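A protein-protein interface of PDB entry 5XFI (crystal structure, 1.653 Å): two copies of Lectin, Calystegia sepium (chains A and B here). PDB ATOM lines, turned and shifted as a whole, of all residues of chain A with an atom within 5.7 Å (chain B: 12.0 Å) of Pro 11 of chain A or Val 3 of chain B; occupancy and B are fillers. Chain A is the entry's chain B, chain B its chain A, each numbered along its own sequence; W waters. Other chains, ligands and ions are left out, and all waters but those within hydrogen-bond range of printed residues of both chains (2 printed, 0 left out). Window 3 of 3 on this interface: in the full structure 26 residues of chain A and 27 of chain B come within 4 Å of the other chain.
The backbone carbonyl oxygen (O) of Ala 2 of chain B lies close to the side-chain amide oxygen (OD1) of Asn 15 of chain A.
O of Pro 4 of chain B is in hydrogen-bond range of NH1 of Arg 138 of chain A, at 2.8 Å.
NE of Arg 138 of chain A sits at hydrogen-bond distance from O of Asn 15 of chain A, at 3.2 Å.
The backbone carbonyl oxygen (O) of Leu 136 of chain A lies within hydrogen-bond range of the backbone NH (N) of Gly 147 of chain A (2.7 Å).
The backbone NH (N) of Arg 138 of chain A is in hydrogen-bond range of the backbone carbonyl oxygen (O) of Ala 145 of chain A (3.1 Å).
Position printed for both chains: 8.
Printed residues of chain A that touch a printed residue of chain B: Pro 11, Gly 13, Asn 14, Asn 15, Leu 136, Arg 138 and Ala 145.
Along chain A the printed residues that touch a printed residue of chain B span positions 11 to 145.
Of the 10 printed residues of chain B, 4 touch a printed residue of chain A.
Hydrophobic or aromatic side chains of chain B that line the printed part of chain A: Val 3, Pro 4 and Met 5.
Among the printed residues, 10 pairs touch across the chains.
Among the printed residues, no Asp or Glu carboxylate lies within 4 Å of a Lys or Arg side-chain nitrogen of the other chain.
No residue of chain B comes within 4 Å of Ser 9 of chain A.
No residue of chain B comes within 4 Å of Gly 10 of chain A.
Printed residues of chain B within 4 Å of Pro 11 of chain A: Val 3.
Of chain B, only Val 3 (3.9 Å) comes within 4 Å of Asn 14 of chain A.
Of chain B, only Met 5 comes within 4 Å of Leu 136 of chain A.
No residue of chain B comes within 4 Å of Gly 137 of chain A.
Arg 138 of chain A touches just these residues of chain B: Val 3 (3.7 Å) and Pro 4 (2.8 Å).
No residue of chain B comes within 4 Å of Gly 147 of chain A.
Printed residues of chain A within 4 Å of Ala 2 of chain B: Asn 15 (3.5 Å).
Of chain A, only Pro 11 (3.9 Å), Gly 13 (3.7 Å), Asn 14 (3.9 Å), Asn 15 (3.4 Å), Arg 138 (3.7 Å) and Ala 145 (3.8 Å) come within 4 Å of Val 3 of chain B.
Printed residues of chain A within 4 Å of Pro 4 of chain B: Asn 15 (3.4 Å) and Arg 138 (2.8 Å).
Of the printed residues of chain A, Met 5 of chain B touches Leu 136 (3.7 Å).
The nearest residue of chain A that does not touch Val 3 of chain B is Trp 12 of chain A (4.5 Å).
The nearest printed residue of chain A that does not touch Met 5 of chain B is Pro 11 of chain A (4.02 Å).
Water W1 lies within hydrogen-bond range of OD1 of Asp 6 of chain B (2.7 Å), NH2 of Arg 138 of chain A (3.1 Å) and NH2 of Arg 23 of chain B (3.5 Å).
Water W2 lies within hydrogen-bond range of the side-chain carboxylate (OD1) of Asp 6 of chain B (2.8 Å) and the guanidinium group (NH1) of Arg 138 of chain A (2.8 Å).
Among the printed residues, merely in contact across the chains: Pro 11 of chain A with Val 3 of chain B (3.9 Å), Gly 13 of chain A with Val 3 of chain B (3.7 Å), Asn 14 of chain A with Val 3 of chain B (3.9 Å), Asn 15 of chain A with Val 3 of chain B (3.4 Å), Asn 15 of chain A with Pro 4 of chain B (3.4 Å), Leu 136 of chain A with Met 5 of chain B (3.7 Å), Arg 138 of chain A with Val 3 of chain B (3.7 Å) and Ala 145 of chain A with Val 3 of chain B (3.8 Å).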
ATOM      1  N   ILE A   8      12.729 -18.021   5.276  1.00  0.00           N
ATOM      2  CA  ILE A   8      13.634 -17.258   6.129  1.00  0.00           C
ATOM      3  C   ILE A   8      13.335 -15.775   5.957  1.00  0.00           C
ATOM      4  O   ILE A   8      13.230 -15.290   4.825  1.00  0.00           O
ATOM      5  CB  ILE A   8      15.103 -17.552   5.770  1.00  0.00           C
ATOM      6  CG1 ILE A   8      15.469 -18.991   6.101  1.00  0.00           C
ATOM      7  CG2 ILE A   8      16.054 -16.477   6.428  1.00  0.00           C
ATOM      8  CD1 ILE A   8      16.798 -19.477   5.446  1.00  0.00           C
ATOM      9  N   SER A   9      13.218 -15.053   7.070  1.00  0.00           N
ATOM     10  CA  SER A   9      13.233 -13.597   7.080  1.00  0.00           C
ATOM     11  C   SER A   9      14.588 -13.123   7.604  1.00  0.00           C
ATOM     12  O   SER A   9      15.095 -13.650   8.593  1.00  0.00           O
ATOM     13  CB  SER A   9      12.094 -13.049   7.936  1.00  0.00           C
ATOM     14  OG  SER A   9      11.977 -11.634   7.816  1.00  0.00           O
ATOM     15  N   GLY A  10      15.186 -12.138   6.939  1.00  0.00           N
ATOM     16  CA  GLY A  10      16.570 -11.816   7.261  1.00  0.00           C
ATOM     17  C   GLY A  10      17.565 -12.842   6.716  1.00  0.00           C
ATOM     18  O   GLY A  10      17.360 -13.441   5.642  1.00  0.00           O
ATOM     19  N   PRO A  11      18.671 -13.085   7.452  1.00  0.00           N
ATOM     20  CA  PRO A  11      19.049 -12.429   8.716  1.00  0.00           C
ATOM     21  C   PRO A  11      19.365 -10.961   8.559  1.00  0.00           C
ATOM     22  O   PRO A  11      19.742 -10.520   7.470  1.00  0.00           O
ATOM     23  CB  PRO A  11      20.343 -13.161   9.128  1.00  0.00           C
ATOM     24  CG  PRO A  11      20.310 -14.438   8.432  1.00  0.00           C
ATOM     25  CD  PRO A  11      19.565 -14.212   7.132  1.00  0.00           C
ATOM     26  N   TRP A  12      19.216 -10.233   9.652  1.00  0.00           N
ATOM     27  CA  TRP A  12      19.659  -8.853   9.772  1.00  0.00           C
ATOM     28  C   TRP A  12      20.936  -8.817  10.607  1.00  0.00           C
ATOM     29  O   TRP A  12      21.136  -9.642  11.501  1.00  0.00           O
ATOM     30  CB  TRP A  12      18.554  -7.999  10.406  1.00  0.00           C
ATOM     31  CG  TRP A  12      17.250  -8.201   9.660  1.00  0.00           C
ATOM     32  CD1 TRP A  12      16.913  -7.663   8.443  1.00  0.00           C
ATOM     33  CD2 TRP A  12      16.141  -9.037  10.043  1.00  0.00           C
ATOM     34  NE1 TRP A  12      15.675  -8.108   8.051  1.00  0.00           N
ATOM     35  CE2 TRP A  12      15.171  -8.941   9.019  1.00  0.00           C
ATOM     36  CE3 TRP A  12      15.871  -9.851  11.152  1.00  0.00           C
ATOM     37  CZ2 TRP A  12      13.958  -9.634   9.063  1.00  0.00           C
ATOM     38  CZ3 TRP A  12      14.664 -10.545  11.189  1.00  0.00           C
ATOM     39  CH2 TRP A  12      13.723 -10.433  10.149  1.00  0.00           C
ATOM     40  N   GLY A  13      21.818  -7.868  10.299  1.00  0.00           N
ATOM     41  CA  GLY A  13      23.055  -7.732  11.032  1.00  0.00           C
ATOM     42  C   GLY A  13      24.263  -7.805  10.110  1.00  0.00           C
ATOM     43  O   GLY A  13      24.207  -7.368   8.953  1.00  0.00           O
ATOM     44  N   ASN A  14      25.337  -8.401  10.625  1.00  0.00           N
ATOM     45  CA  ASN A  14      26.666  -8.327  10.043  1.00  0.00           C
ATOM     46  C   ASN A  14      27.220  -9.720   9.765  1.00  0.00           C
ATOM     47  O   ASN A  14      26.624 -10.739  10.114  1.00  0.00           O
ATOM     48  CB  ASN A  14      27.575  -7.532  10.976  1.00  0.00           C
ATOM     49  CG  ASN A  14      27.032  -6.143  11.223  1.00  0.00           C
ATOM     50  OD1 ASN A  14      26.727  -5.423  10.268  1.00  0.00           O
ATOM     51  ND2 ASN A  14      26.832  -5.788  12.489  1.00  0.00           N
ATOM     52  N   ASN A  15      28.370  -9.762   9.090  1.00  0.00           N
ATOM     53  CA  ASN A  15      28.860 -11.001   8.504  1.00  0.00           C
ATOM     54  C   ASN A  15      29.916 -11.705   9.359  1.00  0.00           C
ATOM     55  O   ASN A  15      30.450 -12.736   8.931  1.00  0.00           O
ATOM     56  CB  ASN A  15      29.401 -10.715   7.092  1.00  0.00           C
ATOM     57  CG  ASN A  15      28.336 -10.074   6.183  1.00  0.00           C
ATOM     58  OD1 ASN A  15      27.142 -10.066   6.505  1.00  0.00           O
ATOM     59  ND2 ASN A  15      28.761  -9.559   5.042  1.00  0.00           N
ATOM     60  N   LEU A 136      17.915 -18.140  13.116  1.00  0.00           N
ATOM     61  CA  LEU A 136      19.213 -18.396  12.509  1.00  0.00           C
ATOM     62  C   LEU A 136      19.997 -17.087  12.543  1.00  0.00           C
ATOM     63  O   LEU A 136      19.454 -16.014  12.839  1.00  0.00           O
ATOM     64  CB  LEU A 136      19.088 -18.952  11.071  1.00  0.00           C
ATOM     65  CG  LEU A 136      18.660 -17.990   9.938  1.00  0.00           C
ATOM     66  CD1 LEU A 136      18.854 -18.709   8.627  1.00  0.00           C
ATOM     67  CD2 LEU A 136      17.200 -17.611  10.103  1.00  0.00           C
ATOM     68  N   GLY A 137      21.301 -17.182  12.315  1.00  0.00           N
ATOM     69  CA  GLY A 137      22.060 -15.951  12.267  1.00  0.00           C
ATOM     70  C   GLY A 137      23.538 -16.244  12.298  1.00  0.00           C
ATOM     71  O   GLY A 137      23.988 -17.275  11.797  1.00  0.00           O
ATOM     72  N   ARG A 138      24.290 -15.305  12.866  1.00  0.00           N
ATOM     73  CA  ARG A 138      25.712 -15.528  13.098  1.00  0.00           C
ATOM     74  C   ARG A 138      26.096 -15.085  14.508  1.00  0.00           C
ATOM     75  O   ARG A 138      25.472 -14.175  15.087  1.00  0.00           O
ATOM     76  CB  ARG A 138      26.573 -14.784  12.079  1.00  0.00           C
ATOM     77  CG  ARG A 138      26.237 -15.115  10.615  1.00  0.00           C
ATOM     78  CD  ARG A 138      27.284 -14.538   9.634  1.00  0.00           C
ATOM     79  NE  ARG A 138      28.560 -15.248   9.731  1.00  0.00           N
ATOM     80  CZ  ARG A 138      28.818 -16.393   9.112  1.00  0.00           C
ATOM     81  NH1 ARG A 138      27.863 -16.968   8.363  1.00  0.00           N
ATOM     82  NH2 ARG A 138      30.027 -16.963   9.247  1.00  0.00           N
ATOM     83  N   ALA A 145      24.357 -11.481  13.895  1.00  0.00           N
ATOM     84  CA  ALA A 145      23.205 -11.388  13.005  1.00  0.00           C
ATOM     85  C   ALA A 145      22.104 -12.312  13.526  1.00  0.00           C
ATOM     86  O   ALA A 145      22.374 -13.310  14.208  1.00  0.00           O
ATOM     87  CB  ALA A 145      23.561 -11.768  11.561  1.00  0.00           C
ATOM     88  N   ILE A 146      20.864 -11.999  13.152  1.00  0.00           N
ATOM     89  CA  ILE A 146      19.736 -12.849  13.527  1.00  0.00           C
ATOM     90  C   ILE A 146      18.639 -12.708  12.482  1.00  0.00           C
ATOM     91  O   ILE A 146      18.383 -11.617  11.963  1.00  0.00           O
ATOM     92  CB  ILE A 146      19.233 -12.530  14.956  1.00  0.00           C
ATOM     93  CG1 ILE A 146      18.163 -13.549  15.390  1.00  0.00           C
ATOM     94  CG2 ILE A 146      18.686 -11.098  15.061  1.00  0.00           C
ATOM     95  CD1 ILE A 146      17.872 -13.525  16.926  1.00  0.00           C
ATOM     96  N   GLY A 147      17.994 -13.829  12.173  1.00  0.00           N
ATOM     97  CA  GLY A 147      16.806 -13.878  11.341  1.00  0.00           C
ATOM     98  C   GLY A 147      15.884 -14.958  11.862  1.00  0.00           C
ATOM     99  O   GLY A 147      16.157 -15.581  12.894  1.00  0.00           O
ATOM    100  N   THR A 148      14.775 -15.170  11.142  1.00  0.00           N
ATOM    101  CA  THR A 148      13.719 -16.082  11.592  1.00  0.00           C
ATOM    102  C   THR A 148      13.359 -17.107  10.523  1.00  0.00           C
ATOM    103  O   THR A 148      13.478 -16.857   9.319  1.00  0.00           O
ATOM    104  CB  THR A 148      12.428 -15.332  11.969  1.00  0.00           C
ATOM    105  OG1 THR A 148      11.962 -14.615  10.812  1.00  0.00           O
ATOM    106  CG2 THR A 148      12.674 -14.379  13.132  1.00  0.00           C
ATOM    107  N   ALA B   2      24.938  -9.234   1.897  1.00  0.00           N
ATOM    108  CA  ALA B   2      23.959  -9.992   2.669  1.00  0.00           C
ATOM    109  C   ALA B   2      24.684 -10.909   3.649  1.00  0.00           C
ATOM    110  O   ALA B   2      25.879 -11.178   3.474  1.00  0.00           O
ATOM    111  CB  ALA B   2      23.043 -10.799   1.745  1.00  0.00           C
ATOM    112  N   VAL B   3      23.965 -11.396   4.662  1.00  0.00           N
ATOM    113  CA  VAL B   3      24.595 -12.163   5.745  1.00  0.00           C
ATOM    114  C   VAL B   3      24.844 -13.580   5.249  1.00  0.00           C
ATOM    115  O   VAL B   3      23.894 -14.258   4.841  1.00  0.00           O
ATOM    116  CB  VAL B   3      23.718 -12.158   7.013  1.00  0.00           C
ATOM    117  CG1 VAL B   3      24.295 -13.107   8.057  1.00  0.00           C
ATOM    118  CG2 VAL B   3      23.614 -10.736   7.603  1.00  0.00           C
ATOM    119  N   PRO B   4      26.092 -14.063   5.233  1.00  0.00           N
ATOM    120  CA  PRO B   4      26.350 -15.411   4.712  1.00  0.00           C
ATOM    121  C   PRO B   4      25.759 -16.474   5.618  1.00  0.00           C
ATOM    122  O   PRO B   4      25.633 -16.289   6.829  1.00  0.00           O
ATOM    123  CB  PRO B   4      27.884 -15.506   4.673  1.00  0.00           C
ATOM    124  CG  PRO B   4      28.362 -14.466   5.633  1.00  0.00           C
ATOM    125  CD  PRO B   4      27.310 -13.392   5.712  1.00  0.00           C
ATOM    126  N   MET B   5      25.349 -17.578   4.998  1.00  0.00           N
ATOM    127  CA  MET B   5      24.869 -18.757   5.701  1.00  0.00           C
ATOM    128  C   MET B   5      25.634 -19.953   5.162  1.00  0.00           C
ATOM    129  O   MET B   5      26.052 -19.951   4.002  1.00  0.00           O
ATOM    130  CB  MET B   5      23.348 -18.926   5.518  1.00  0.00           C
ATOM    131  CG  MET B   5      22.592 -17.660   5.906  1.00  0.00           C
ATOM    132  SD  MET B   5      20.809 -17.749   5.688  1.00  0.00           S
ATOM    133  CE  MET B   5      20.691 -17.980   3.910  1.00  0.00           C
ATOM    134  N   ASP B   6      25.828 -20.972   6.002  1.00  0.00           N
ATOM    135  CA  ASP B   6      26.612 -22.127   5.570  1.00  0.00           C
ATOM    136  C   ASP B   6      25.904 -22.897   4.456  1.00  0.00           C
ATOM    137  O   ASP B   6      24.684 -23.092   4.478  1.00  0.00           O
ATOM    138  CB  ASP B   6      26.903 -23.079   6.729  1.00  0.00           C
ATOM    139  CG  ASP B   6      27.850 -22.480   7.757  1.00  0.00           C
ATOM    140  OD1 ASP B   6      28.614 -21.526   7.431  1.00  0.00           O
ATOM    141  OD2 ASP B   6      27.830 -22.979   8.898  1.00  0.00           O
ATOM    142  N   THR B   7      26.694 -23.390   3.502  1.00  0.00           N
ATOM    143  CA  THR B   7      26.107 -24.032   2.335  1.00  0.00           C
ATOM    144  C   THR B   7      25.393 -25.329   2.708  1.00  0.00           C
ATOM    145  O   THR B   7      25.868 -26.122   3.529  1.00  0.00           O
ATOM    146  CB  THR B   7      27.179 -24.266   1.263  1.00  0.00           C
ATOM    147  OG1 THR B   7      26.547 -24.739   0.070  1.00  0.00           O
ATOM    148  CG2 THR B   7      28.208 -25.245   1.722  1.00  0.00           C
ATOM    149  N   ILE B   8      24.210 -25.508   2.132  1.00  0.00           N
ATOM    150  CA  ILE B   8      23.357 -26.659   2.411  1.00  0.00           C
ATOM    151  C   ILE B   8      23.579 -27.724   1.348  1.00  0.00           C
ATOM    152  O   ILE B   8      23.563 -27.425   0.150  1.00  0.00           O
ATOM    153  CB  ILE B   8      21.875 -26.233   2.451  1.00  0.00           C
ATOM    154  CG1 ILE B   8      21.620 -25.292   3.618  1.00  0.00           C
ATOM    155  CG2 ILE B   8      20.938 -27.488   2.445  1.00  0.00           C
ATOM    156  CD1 ILE B   8      20.261 -24.539   3.540  1.00  0.00           C
ATOM    157  N   SER B  21      15.894 -27.685  11.873  1.00  0.00           N
ATOM    158  CA  SER B  21      17.254 -27.240  11.567  1.00  0.00           C
ATOM    159  C   SER B  21      18.089 -27.128  12.839  1.00  0.00           C
ATOM    160  O   SER B  21      17.607 -26.636  13.870  1.00  0.00           O
ATOM    161  CB  SER B  21      17.209 -25.889  10.832  1.00  0.00           C
ATOM    162  OG  SER B  21      18.522 -25.449  10.477  1.00  0.00           O
ATOM    163  N   ARG B  23      22.188 -26.057  13.616  1.00  0.00           N
ATOM    164  CA  ARG B  23      23.598 -25.755  13.367  1.00  0.00           C
ATOM    165  C   ARG B  23      24.107 -25.025  14.604  1.00  0.00           C
ATOM    166  O   ARG B  23      23.960 -23.794  14.716  1.00  0.00           O
ATOM    167  CB  ARG B  23      23.763 -24.919  12.097  1.00  0.00           C
ATOM    168  CG  ARG B  23      25.155 -24.995  11.449  1.00  0.00           C
ATOM    169  CD  ARG B  23      26.240 -24.401  12.340  1.00  0.00           C
ATOM    170  NE  ARG B  23      27.353 -23.888  11.563  1.00  0.00           N
ATOM    171  CZ  ARG B  23      28.504 -23.476  12.069  1.00  0.00           C
ATOM    172  NH1 ARG B  23      28.754 -23.548  13.387  1.00  0.00           N
ATOM    173  NH2 ARG B  23      29.426 -22.991  11.236  1.00  0.00           N
ATOM    174  N   TYR B 149      24.548 -28.811   6.823  1.00  0.00           N
ATOM    175  CA  TYR B 149      25.244 -27.535   6.728  1.00  0.00           C
ATOM    176  C   TYR B 149      26.740 -27.819   6.683  1.00  0.00           C
ATOM    177  O   TYR B 149      27.224 -28.720   7.375  1.00  0.00           O
ATOM    178  CB  TYR B 149      24.951 -26.617   7.928  1.00  0.00           C
ATOM    179  CG  TYR B 149      23.531 -26.130   7.962  1.00  0.00           C
ATOM    180  CD1 TYR B 149      23.086 -25.132   7.101  1.00  0.00           C
ATOM    181  CD2 TYR B 149      22.638 -26.651   8.886  1.00  0.00           C
ATOM    182  CE1 TYR B 149      21.762 -24.692   7.143  1.00  0.00           C
ATOM    183  CE2 TYR B 149      21.325 -26.216   8.937  1.00  0.00           C
ATOM    184  CZ  TYR B 149      20.903 -25.228   8.080  1.00  0.00           C
ATOM    185  OH  TYR B 149      19.573 -24.799   8.125  1.00  0.00           O
HETATM  186  O   HOH W   1      29.819 -20.053   9.411  1.00  0.00           O
HETATM  187  O   HOH W   2      28.572 -18.900   6.412  1.00  0.00           O
